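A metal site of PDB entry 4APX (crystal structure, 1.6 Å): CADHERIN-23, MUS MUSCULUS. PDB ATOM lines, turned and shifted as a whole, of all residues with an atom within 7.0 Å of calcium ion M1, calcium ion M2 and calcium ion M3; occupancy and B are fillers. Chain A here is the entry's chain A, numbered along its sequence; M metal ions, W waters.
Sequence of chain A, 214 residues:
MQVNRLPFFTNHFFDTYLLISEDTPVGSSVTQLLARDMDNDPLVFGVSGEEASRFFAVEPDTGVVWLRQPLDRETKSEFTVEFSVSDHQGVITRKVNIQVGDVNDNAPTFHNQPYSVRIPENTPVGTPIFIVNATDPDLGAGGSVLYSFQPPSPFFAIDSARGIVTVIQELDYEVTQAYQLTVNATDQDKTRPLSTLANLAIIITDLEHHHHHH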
ATOM      1  N   GLU A  22     -10.824  -9.353  -7.384  1.00  0.00           N
ATOM      2  CA  GLU A  22      -9.994  -8.762  -6.315  1.00  0.00           C
ATOM      3  C   GLU A  22      -9.707  -7.260  -6.469  1.00  0.00           C
ATOM      4  O   GLU A  22      -9.301  -6.642  -5.491  1.00  0.00           O
ATOM      5  CB  GLU A  22      -8.661  -9.527  -6.130  1.00  0.00           C
ATOM      6  CG  GLU A  22      -7.725  -9.427  -7.287  1.00  0.00           C
ATOM      7  CD  GLU A  22      -6.378 -10.049  -7.014  1.00  0.00           C
ATOM      8  OE1 GLU A  22      -5.947 -10.053  -5.813  1.00  0.00           O
ATOM      9  OE2 GLU A  22      -5.732 -10.492  -7.997  1.00  0.00           O
ATOM     10  N   LEU A  71     -10.127  -7.028  -1.193  1.00  0.00           N
ATOM     11  CA  LEU A  71      -9.945  -8.456  -1.366  1.00  0.00           C
ATOM     12  C   LEU A  71      -8.537  -8.654  -1.926  1.00  0.00           C
ATOM     13  O   LEU A  71      -7.910  -7.706  -2.421  1.00  0.00           O
ATOM     14  CB  LEU A  71     -10.992  -9.040  -2.317  1.00  0.00           C
ATOM     15  CG  LEU A  71     -12.452  -9.036  -1.864  1.00  0.00           C
ATOM     16  CD1 LEU A  71     -13.364  -9.425  -3.018  1.00  0.00           C
ATOM     17  CD2 LEU A  71     -12.692  -9.944  -0.679  1.00  0.00           C
ATOM     18  N   ASP A  72      -7.991  -9.845  -1.771  1.00  0.00           N
ATOM     19  CA  ASP A  72      -6.666 -10.160  -2.325  1.00  0.00           C
ATOM     20  C   ASP A  72      -6.636 -11.639  -2.573  1.00  0.00           C
ATOM     21  O   ASP A  72      -6.474 -12.417  -1.639  1.00  0.00           O
ATOM     22  CB  ASP A  72      -5.532  -9.729  -1.374  1.00  0.00           C
ATOM     23  CG  ASP A  72      -4.166 -10.159  -1.873  1.00  0.00           C
ATOM     24  OD1 ASP A  72      -4.043 -10.550  -3.065  1.00  0.00           O
ATOM     25  OD2 ASP A  72      -3.211 -10.109  -1.089  1.00  0.00           O
ATOM     26  N   ARG A  73      -6.755 -12.027  -3.848  1.00  0.00           N
ATOM     27  CA  ARG A  73      -6.815 -13.409  -4.231  1.00  0.00           C
ATOM     28  C   ARG A  73      -5.564 -14.181  -3.803  1.00  0.00           C
ATOM     29  O   ARG A  73      -5.635 -15.376  -3.515  1.00  0.00           O
ATOM     30  CB  ARG A  73      -6.990 -13.554  -5.738  1.00  0.00           C
ATOM     31  CG  ARG A  73      -7.376 -14.971  -6.167  1.00  0.00           C
ATOM     32  CD  ARG A  73      -7.079 -15.281  -7.578  1.00  0.00           C
ATOM     33  NE  ARG A  73      -5.623 -15.293  -7.779  1.00  0.00           N
ATOM     34  CZ  ARG A  73      -4.827 -16.333  -7.563  1.00  0.00           C
ATOM     35  NH1 ARG A  73      -5.292 -17.527  -7.199  1.00  0.00           N
ATOM     36  NH2 ARG A  73      -3.526 -16.179  -7.748  1.00  0.00           N
ATOM     37  N   GLU A  74      -4.426 -13.483  -3.773  1.00  0.00           N
ATOM     38  CA  GLU A  74      -3.162 -14.097  -3.359  1.00  0.00           C
ATOM     39  C   GLU A  74      -3.060 -14.286  -1.834  1.00  0.00           C
ATOM     40  O   GLU A  74      -2.172 -15.042  -1.371  1.00  0.00           O
ATOM     41  CB  GLU A  74      -1.981 -13.274  -3.863  1.00  0.00           C
ATOM     42  CG  GLU A  74      -1.670 -13.441  -5.339  1.00  0.00           C
ATOM     43  CD  GLU A  74      -2.657 -12.741  -6.267  1.00  0.00           C
ATOM     44  OE1 GLU A  74      -3.064 -11.586  -6.019  1.00  0.00           O
ATOM     45  OE2 GLU A  74      -2.954 -13.313  -7.341  1.00  0.00           O
ATOM     46  N   THR A  75      -3.904 -13.602  -1.057  1.00  0.00           N
ATOM     47  CA  THR A  75      -3.927 -13.744   0.429  1.00  0.00           C
ATOM     48  C   THR A  75      -5.065 -14.693   0.830  1.00  0.00           C
ATOM     49  O   THR A  75      -4.896 -15.538   1.726  1.00  0.00           O
ATOM     50  CB  THR A  75      -4.062 -12.383   1.147  1.00  0.00           C
ATOM     51  OG1 THR A  75      -2.827 -11.665   1.017  1.00  0.00           O
ATOM     52  CG2 THR A  75      -4.336 -12.562   2.633  1.00  0.00           C
ATOM     53  N   GLY A 101     -11.941 -13.285  -7.874  1.00  0.00           N
ATOM     54  CA  GLY A 101     -11.401 -13.305  -9.222  1.00  0.00           C
ATOM     55  C   GLY A 101     -10.019 -12.678  -9.263  1.00  0.00           C
ATOM     56  O   GLY A 101      -9.736 -11.728  -8.528  1.00  0.00           O
ATOM     57  N   ASP A 102      -9.157 -13.207 -10.113  1.00  0.00           N
ATOM     58  CA  ASP A 102      -7.791 -12.708 -10.190  1.00  0.00           C
ATOM     59  C   ASP A 102      -7.647 -11.528 -11.127  1.00  0.00           C
ATOM     60  O   ASP A 102      -8.351 -11.432 -12.141  1.00  0.00           O
ATOM     61  CB  ASP A 102      -6.838 -13.816 -10.685  1.00  0.00           C
ATOM     62  CG  ASP A 102      -5.378 -13.435 -10.547  1.00  0.00           C
ATOM     63  OD1 ASP A 102      -4.946 -13.046  -9.427  1.00  0.00           O
ATOM     64  OD2 ASP A 102      -4.631 -13.513 -11.537  1.00  0.00           O
ATOM     65  N   VAL A 103      -6.750 -10.627 -10.766  1.00  0.00           N
ATOM     66  CA  VAL A 103      -6.233  -9.651 -11.706  1.00  0.00           C
ATOM     67  C   VAL A 103      -4.722  -9.718 -11.605  1.00  0.00           C
ATOM     68  O   VAL A 103      -4.187 -10.206 -10.617  1.00  0.00           O
ATOM     69  CB  VAL A 103      -6.749  -8.249 -11.497  1.00  0.00           C
ATOM     70  CG1 VAL A 103      -8.284  -8.208 -11.483  1.00  0.00           C
ATOM     71  CG2 VAL A 103      -6.192  -7.655 -10.219  1.00  0.00           C
ATOM     72  N   ASN A 104      -4.027  -9.278 -12.640  1.00  0.00           N
ATOM     73  CA  ASN A 104      -2.564  -9.254 -12.581  1.00  0.00           C
ATOM     74  C   ASN A 104      -2.146  -8.097 -11.692  1.00  0.00           C
ATOM     75  O   ASN A 104      -2.214  -6.936 -12.102  1.00  0.00           O
ATOM     76  CB  ASN A 104      -1.940  -9.134 -13.981  1.00  0.00           C
ATOM     77  CG  ASN A 104      -0.449  -9.313 -13.935  1.00  0.00           C
ATOM     78  OD1 ASN A 104       0.007 -10.289 -13.341  1.00  0.00           O
ATOM     79  ND2 ASN A 104       0.314  -8.371 -14.473  1.00  0.00           N
ATOM     80  N   ASP A 105      -1.762  -8.416 -10.456  1.00  0.00           N
ATOM     81  CA  ASP A 105      -1.354  -7.358  -9.525  1.00  0.00           C
ATOM     82  C   ASP A 105      -0.044  -7.612  -8.804  1.00  0.00           C
ATOM     83  O   ASP A 105       0.311  -6.851  -7.881  1.00  0.00           O
ATOM     84  CB  ASP A 105      -2.498  -6.945  -8.567  1.00  0.00           C
ATOM     85  CG  ASP A 105      -3.029  -8.071  -7.699  1.00  0.00           C
ATOM     86  OD1 ASP A 105      -2.678  -9.246  -7.907  1.00  0.00           O
ATOM     87  OD2 ASP A 105      -3.832  -7.779  -6.762  1.00  0.00           O
ATOM     88  N   ASN A 106       0.709  -8.627  -9.242  1.00  0.00           N
ATOM     89  CA  ASN A 106       2.036  -8.893  -8.744  1.00  0.00           C
ATOM     90  C   ASN A 106       3.063  -8.908  -9.862  1.00  0.00           C
ATOM     91  O   ASN A 106       2.796  -9.397 -10.954  1.00  0.00           O
ATOM     92  CB  ASN A 106       2.127 -10.253  -8.018  1.00  0.00           C
ATOM     93  CG  ASN A 106       1.289 -10.293  -6.773  1.00  0.00           C
ATOM     94  OD1 ASN A 106       1.818 -10.066  -5.663  1.00  0.00           O
ATOM     95  ND2 ASN A 106      -0.025 -10.531  -6.916  1.00  0.00           N
ATOM     96  N   ALA A 107       4.242  -8.388  -9.558  1.00  0.00           N
ATOM     97  CA  ALA A 107       5.379  -8.506 -10.440  1.00  0.00           C
ATOM     98  C   ALA A 107       6.140  -9.755 -10.024  1.00  0.00           C
ATOM     99  O   ALA A 107       5.978 -10.240  -8.892  1.00  0.00           O
ATOM    100  CB  ALA A 107       6.287  -7.283 -10.373  1.00  0.00           C
ATOM    101  N   PRO A 108       6.980 -10.301 -10.928  1.00  0.00           N
ATOM    102  CA  PRO A 108       7.790 -11.456 -10.529  1.00  0.00           C
ATOM    103  C   PRO A 108       8.802 -11.166  -9.419  1.00  0.00           C
ATOM    104  O   PRO A 108       9.212 -10.019  -9.213  1.00  0.00           O
ATOM    105  CB  PRO A 108       8.525 -11.846 -11.816  1.00  0.00           C
ATOM    106  CG  PRO A 108       7.668 -11.257 -12.920  1.00  0.00           C
ATOM    107  CD  PRO A 108       7.134  -9.997 -12.364  1.00  0.00           C
ATOM    108  N   ASP A 136       5.906 -15.794 -10.048  1.00  0.00           N
ATOM    109  CA  ASP A 136       4.865 -14.772 -10.018  1.00  0.00           C
ATOM    110  C   ASP A 136       3.554 -15.447  -9.684  1.00  0.00           C
ATOM    111  O   ASP A 136       3.169 -16.397 -10.385  1.00  0.00           O
ATOM    112  CB  ASP A 136       4.835 -14.114 -11.395  1.00  0.00           C
ATOM    113  CG  ASP A 136       3.883 -12.911 -11.487  1.00  0.00           C
ATOM    114  OD1 ASP A 136       2.755 -12.943 -10.919  1.00  0.00           O
ATOM    115  OD2 ASP A 136       4.242 -11.926 -12.178  1.00  0.00           O
ATOM    116  N   PRO A 137       2.863 -14.993  -8.621  1.00  0.00           N
ATOM    117  CA  PRO A 137       1.688 -15.688  -8.101  1.00  0.00           C
ATOM    118  C   PRO A 137       0.359 -15.472  -8.796  1.00  0.00           C
ATOM    119  O   PRO A 137      -0.612 -16.156  -8.468  1.00  0.00           O
ATOM    120  CB  PRO A 137       1.595 -15.156  -6.662  1.00  0.00           C
ATOM    121  CG  PRO A 137       2.054 -13.757  -6.776  1.00  0.00           C
ATOM    122  CD  PRO A 137       3.231 -13.857  -7.751  1.00  0.00           C
ATOM    123  N   ASP A 138       0.299 -14.542  -9.737  1.00  0.00           N
ATOM    124  CA  ASP A 138      -0.947 -14.282 -10.447  1.00  0.00           C
ATOM    125  C   ASP A 138      -1.284 -15.446 -11.349  1.00  0.00           C
ATOM    126  O   ASP A 138      -0.414 -16.261 -11.670  1.00  0.00           O
ATOM    127  CB  ASP A 138      -0.814 -13.022 -11.258  1.00  0.00           C
ATOM    128  CG  ASP A 138      -0.656 -11.772 -10.396  1.00  0.00           C
ATOM    129  OD1 ASP A 138      -1.524 -11.504  -9.530  1.00  0.00           O
ATOM    130  OD2 ASP A 138       0.324 -11.063 -10.623  1.00  0.00           O
ATOM    131  N   LEU A 139      -2.542 -15.532 -11.764  1.00  0.00           N
ATOM    132  CA  LEU A 139      -2.988 -16.645 -12.607  1.00  0.00           C
ATOM    133  C   LEU A 139      -2.671 -16.459 -14.075  1.00  0.00           C
ATOM    134  O   LEU A 139      -2.576 -15.318 -14.579  1.00  0.00           O
ATOM    135  CB  LEU A 139      -4.506 -16.845 -12.477  1.00  0.00           C
ATOM    136  CG  LEU A 139      -5.079 -17.257 -11.111  1.00  0.00           C
ATOM    137  CD1 LEU A 139      -6.584 -17.507 -11.170  1.00  0.00           C
ATOM    138  CD2 LEU A 139      -4.350 -18.483 -10.602  1.00  0.00           C
ATOM    139  N   ALA A 141      -1.531 -15.971 -17.771  1.00  0.00           N
ATOM    140  CA  ALA A 141      -0.463 -15.193 -18.403  1.00  0.00           C
ATOM    141  C   ALA A 141       0.210 -14.264 -17.416  1.00  0.00           C
ATOM    142  O   ALA A 141       1.415 -14.025 -17.493  1.00  0.00           O
ATOM    143  CB  ALA A 141      -1.012 -14.407 -19.595  1.00  0.00           C
ATOM    144  N   GLY A 142      -0.560 -13.749 -16.473  1.00  0.00           N
ATOM    145  CA  GLY A 142      -0.033 -12.921 -15.385  1.00  0.00           C
ATOM    146  C   GLY A 142       0.951 -13.588 -14.461  1.00  0.00           C
ATOM    147  O   GLY A 142       1.642 -12.900 -13.710  1.00  0.00           O
ATOM    148  N   GLY A 143       1.046 -14.918 -14.502  1.00  0.00           N
ATOM    149  CA  GLY A 143       1.983 -15.661 -13.699  1.00  0.00           C
ATOM    150  C   GLY A 143       3.083 -16.361 -14.463  1.00  0.00           C
ATOM    151  O   GLY A 143       3.876 -17.096 -13.872  1.00  0.00           O
ATOM    152  N   SER A 144       3.128 -16.167 -15.782  1.00  0.00           N
ATOM    153  CA  SER A 144       4.099 -16.843 -16.654  1.00  0.00           C
ATOM    154  C   SER A 144       5.194 -15.859 -16.976  1.00  0.00           C
ATOM    155  O   SER A 144       4.940 -14.814 -17.568  1.00  0.00           O
ATOM    156  CB  SER A 144       3.408 -17.354 -17.916  1.00  0.00           C
ATOM    157  OG  SER A 144       4.307 -18.073 -18.753  1.00  0.00           O
ATOM    158  N   THR A 186       9.516 -10.495 -16.622  1.00  0.00           N
ATOM    159  CA  THR A 186       8.171  -9.927 -16.799  1.00  0.00           C
ATOM    160  C   THR A 186       7.141 -11.007 -16.872  1.00  0.00           C
ATOM    161  O   THR A 186       7.400 -12.095 -17.361  1.00  0.00           O
ATOM    162  CB  THR A 186       8.077  -9.051 -18.087  1.00  0.00           C
ATOM    163  OG1 THR A 186       6.789  -8.415 -18.153  1.00  0.00           O
ATOM    164  CG2 THR A 186       8.288  -9.894 -19.363  1.00  0.00           C
ATOM    165  N   ASP A 187       5.939 -10.730 -16.364  1.00  0.00           N
ATOM    166  CA  ASP A 187       4.821 -11.602 -16.641  1.00  0.00           C
ATOM    167  C   ASP A 187       4.295 -11.249 -18.045  1.00  0.00           C
ATOM    168  O   ASP A 187       4.849 -10.344 -18.703  1.00  0.00           O
ATOM    169  CB  ASP A 187       3.740 -11.556 -15.555  1.00  0.00           C
ATOM    170  CG  ASP A 187       3.101 -10.230 -15.406  1.00  0.00           C
ATOM    171  OD1 ASP A 187       2.834  -9.573 -16.420  1.00  0.00           O
ATOM    172  OD2 ASP A 187       2.820  -9.843 -14.240  1.00  0.00           O
ATOM    173  N   GLN A 188       3.280 -11.983 -18.497  1.00  0.00           N
ATOM    174  CA  GLN A 188       2.741 -11.824 -19.845  1.00  0.00           C
ATOM    175  C   GLN A 188       1.279 -11.359 -19.870  1.00  0.00           C
ATOM    176  O   GLN A 188       0.547 -11.619 -20.823  1.00  0.00           O
ATOM    177  CB  GLN A 188       2.895 -13.138 -20.605  1.00  0.00           C
ATOM    178  CG  GLN A 188       4.345 -13.495 -20.830  1.00  0.00           C
ATOM    179  CD  GLN A 188       4.496 -14.818 -21.491  1.00  0.00           C
ATOM    180  OE1 GLN A 188       4.417 -14.919 -22.725  1.00  0.00           O
ATOM    181  NE2 GLN A 188       4.698 -15.862 -20.683  1.00  0.00           N
ATOM    182  N   ASP A 189       0.867 -10.638 -18.850  1.00  0.00           N
ATOM    183  CA  ASP A 189      -0.479 -10.120 -18.801  1.00  0.00           C
ATOM    184  C   ASP A 189      -0.710  -9.245 -20.030  1.00  0.00           C
ATOM    185  O   ASP A 189       0.157  -8.471 -20.414  1.00  0.00           O
ATOM    186  CB  ASP A 189      -0.762  -9.315 -17.552  1.00  0.00           C
ATOM    187  CG  ASP A 189      -2.215  -8.914 -17.454  1.00  0.00           C
ATOM    188  OD1 ASP A 189      -3.085  -9.825 -17.351  1.00  0.00           O
ATOM    189  OD2 ASP A 189      -2.500  -7.699 -17.512  1.00  0.00           O
ATOM    190  N   ARG A 192      -1.796  -5.227 -18.592  1.00  0.00           N
ATOM    191  CA  ARG A 192      -0.987  -4.634 -17.517  1.00  0.00           C
ATOM    192  C   ARG A 192       0.147  -5.571 -17.094  1.00  0.00           C
ATOM    193  O   ARG A 192       0.186  -6.020 -15.943  1.00  0.00           O
ATOM    194  CB  ARG A 192      -1.859  -4.289 -16.313  1.00  0.00           C
ATOM    195  CG  ARG A 192      -2.939  -3.205 -16.594  1.00  0.00           C
ATOM    196  CD  ARG A 192      -3.757  -2.809 -15.365  1.00  0.00           C
ATOM    197  NE  ARG A 192      -2.940  -2.347 -14.262  1.00  0.00           N
ATOM    198  CZ  ARG A 192      -2.491  -3.090 -13.245  1.00  0.00           C
ATOM    199  NH1 ARG A 192      -2.817  -4.378 -13.138  1.00  0.00           N
ATOM    200  NH2 ARG A 192      -1.700  -2.537 -12.343  1.00  0.00           N
ATOM    201  N   PRO A 193       1.077  -5.841 -18.004  1.00  0.00           N
ATOM    202  CA  PRO A 193       2.219  -6.658 -17.632  1.00  0.00           C
ATOM    203  C   PRO A 193       3.085  -5.975 -16.564  1.00  0.00           C
ATOM    204  O   PRO A 193       3.242  -4.758 -16.588  1.00  0.00           O
ATOM    205  CB  PRO A 193       2.990  -6.792 -18.931  1.00  0.00           C
ATOM    206  CG  PRO A 193       2.667  -5.496 -19.662  1.00  0.00           C
ATOM    207  CD  PRO A 193       1.212  -5.329 -19.387  1.00  0.00           C
ATOM    208  N   LEU A 194       3.589  -6.775 -15.642  1.00  0.00           N
ATOM    209  CA  LEU A 194       4.400  -6.285 -14.552  1.00  0.00           C
ATOM    210  C   LEU A 194       5.751  -6.974 -14.586  1.00  0.00           C
ATOM    211  O   LEU A 194       5.846  -8.147 -14.929  1.00  0.00           O
ATOM    212  CB  LEU A 194       3.699  -6.518 -13.221  1.00  0.00           C
ATOM    213  CG  LEU A 194       2.388  -5.730 -13.062  1.00  0.00           C
ATOM    214  CD1 LEU A 194       1.675  -6.163 -11.814  1.00  0.00           C
ATOM    215  CD2 LEU A 194       2.641  -4.235 -13.060  1.00  0.00           C
HETATM  216 CA    CA M   1       2.037 -11.055 -12.328  1.00  0.00          CA
HETATM  217 CA    CA M   2      -3.611 -11.351  -8.585  1.00  0.00          CA
HETATM  218 CA    CA M   3      -3.733  -9.538  -5.170  1.00  0.00          CA
HETATM  219  O   HOH W   1      -1.451  -9.136  -4.599  1.00  0.00           O
HETATM  220  O   HOH W   2      -4.368  -7.688  -3.788  1.00  0.00           O
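The side-chain amide nitrogen (ND2) of Asn 106 sits close to the side-chain carboxylate (OE1) of Glu 74 (3.3 Å).
OD1 of Asp 105 sits close to ND2 of Asn 106 (3.1 Å).
The backbone NH (N) of Gly 143 sits close to the backbone carbonyl oxygen (O) of Asp 138, at 3.5 Å.
OD2 of Asp 102 is in hydrogen-bond range of N of Leu 139.
The side-chain carboxylate (OD2) of Asp 72 is in hydrogen-bond range of the side-chain hydroxyl (OG1) of Thr 75, at 2.6 Å.
O of Arg 192 lies within hydrogen-bond range of ND2 of Asn 104.
The backbone NH (N) of Asp 187 is in hydrogen-bond range of the backbone carbonyl oxygen (O) of Leu 194 (3.0 Å).
The backbone NH (N) of Asp 189 sits at hydrogen-bond distance from the side-chain carboxylate (OD1) of Asp 187, 3.3 Å away.
Within 4 Å of calcium ion M1: Asn 104, Asn 106, Asp 136, Asp 138, Gly 142 and Asp 187.
Within 4 Å of calcium ion M2: Glu 22, Glu 74, Asp 102, Val 103, Asp 105 and Asp 138.
Along chain A the residues within 4 Å of calcium ion M2 span positions 22 to 138.
The nearest printed residue that does not touch calcium ion M2 is Asn 106 (4.04 Å).
Within 4 Å of calcium ion M3: Glu 22, Asp 72, Glu 74 and Asp 105.
The nearest printed residue that does not touch calcium ion M3 is Arg 73 (4.1 Å).
Calcium ion M1 is bound by O of Asn 106 (2.3 Å), O of Gly 142 (2.3 Å), OD2 of Asp 136 (2.4 Å), OD1 of Asn 104 (2.4 Å), OD2 of Asp 187 (2.4 Å), OD2 of Asp 138 (2.4 Å) and OD1 of Asp 136 (2.5 Å).
Calcium ion M1 has seven donor atoms within binding distance.
Calcium ion M2 is bound by OD1 of Asp 138 (2.3 Å), OD1 of Asp 102 (2.3 Å), OE2 of Glu 22 (2.4 Å), OD1 of Asp 105 (2.4 Å), O of Val 103 (2.4 Å), OE2 of Glu 74 (2.4 Å) and OE1 of Glu 74 (2.6 Å).
Calcium ion M2 has seven donor atoms within binding distance.
Calcium ion M3 is bound by the side-chain carboxylate of Glu 74 (2.3 Å), the side-chain carboxylate of Asp 72 (2.4 Å), the side-chain carboxylate of Glu 22 (2.4 Å), the side-chain carboxylate of Asp 105 (2.4 Å), water W1 (2.4 Å) and water W2 (2.4 Å).
Slightly farther from calcium ion M3 lies OD1 of Asp 105 (2.9 Å).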
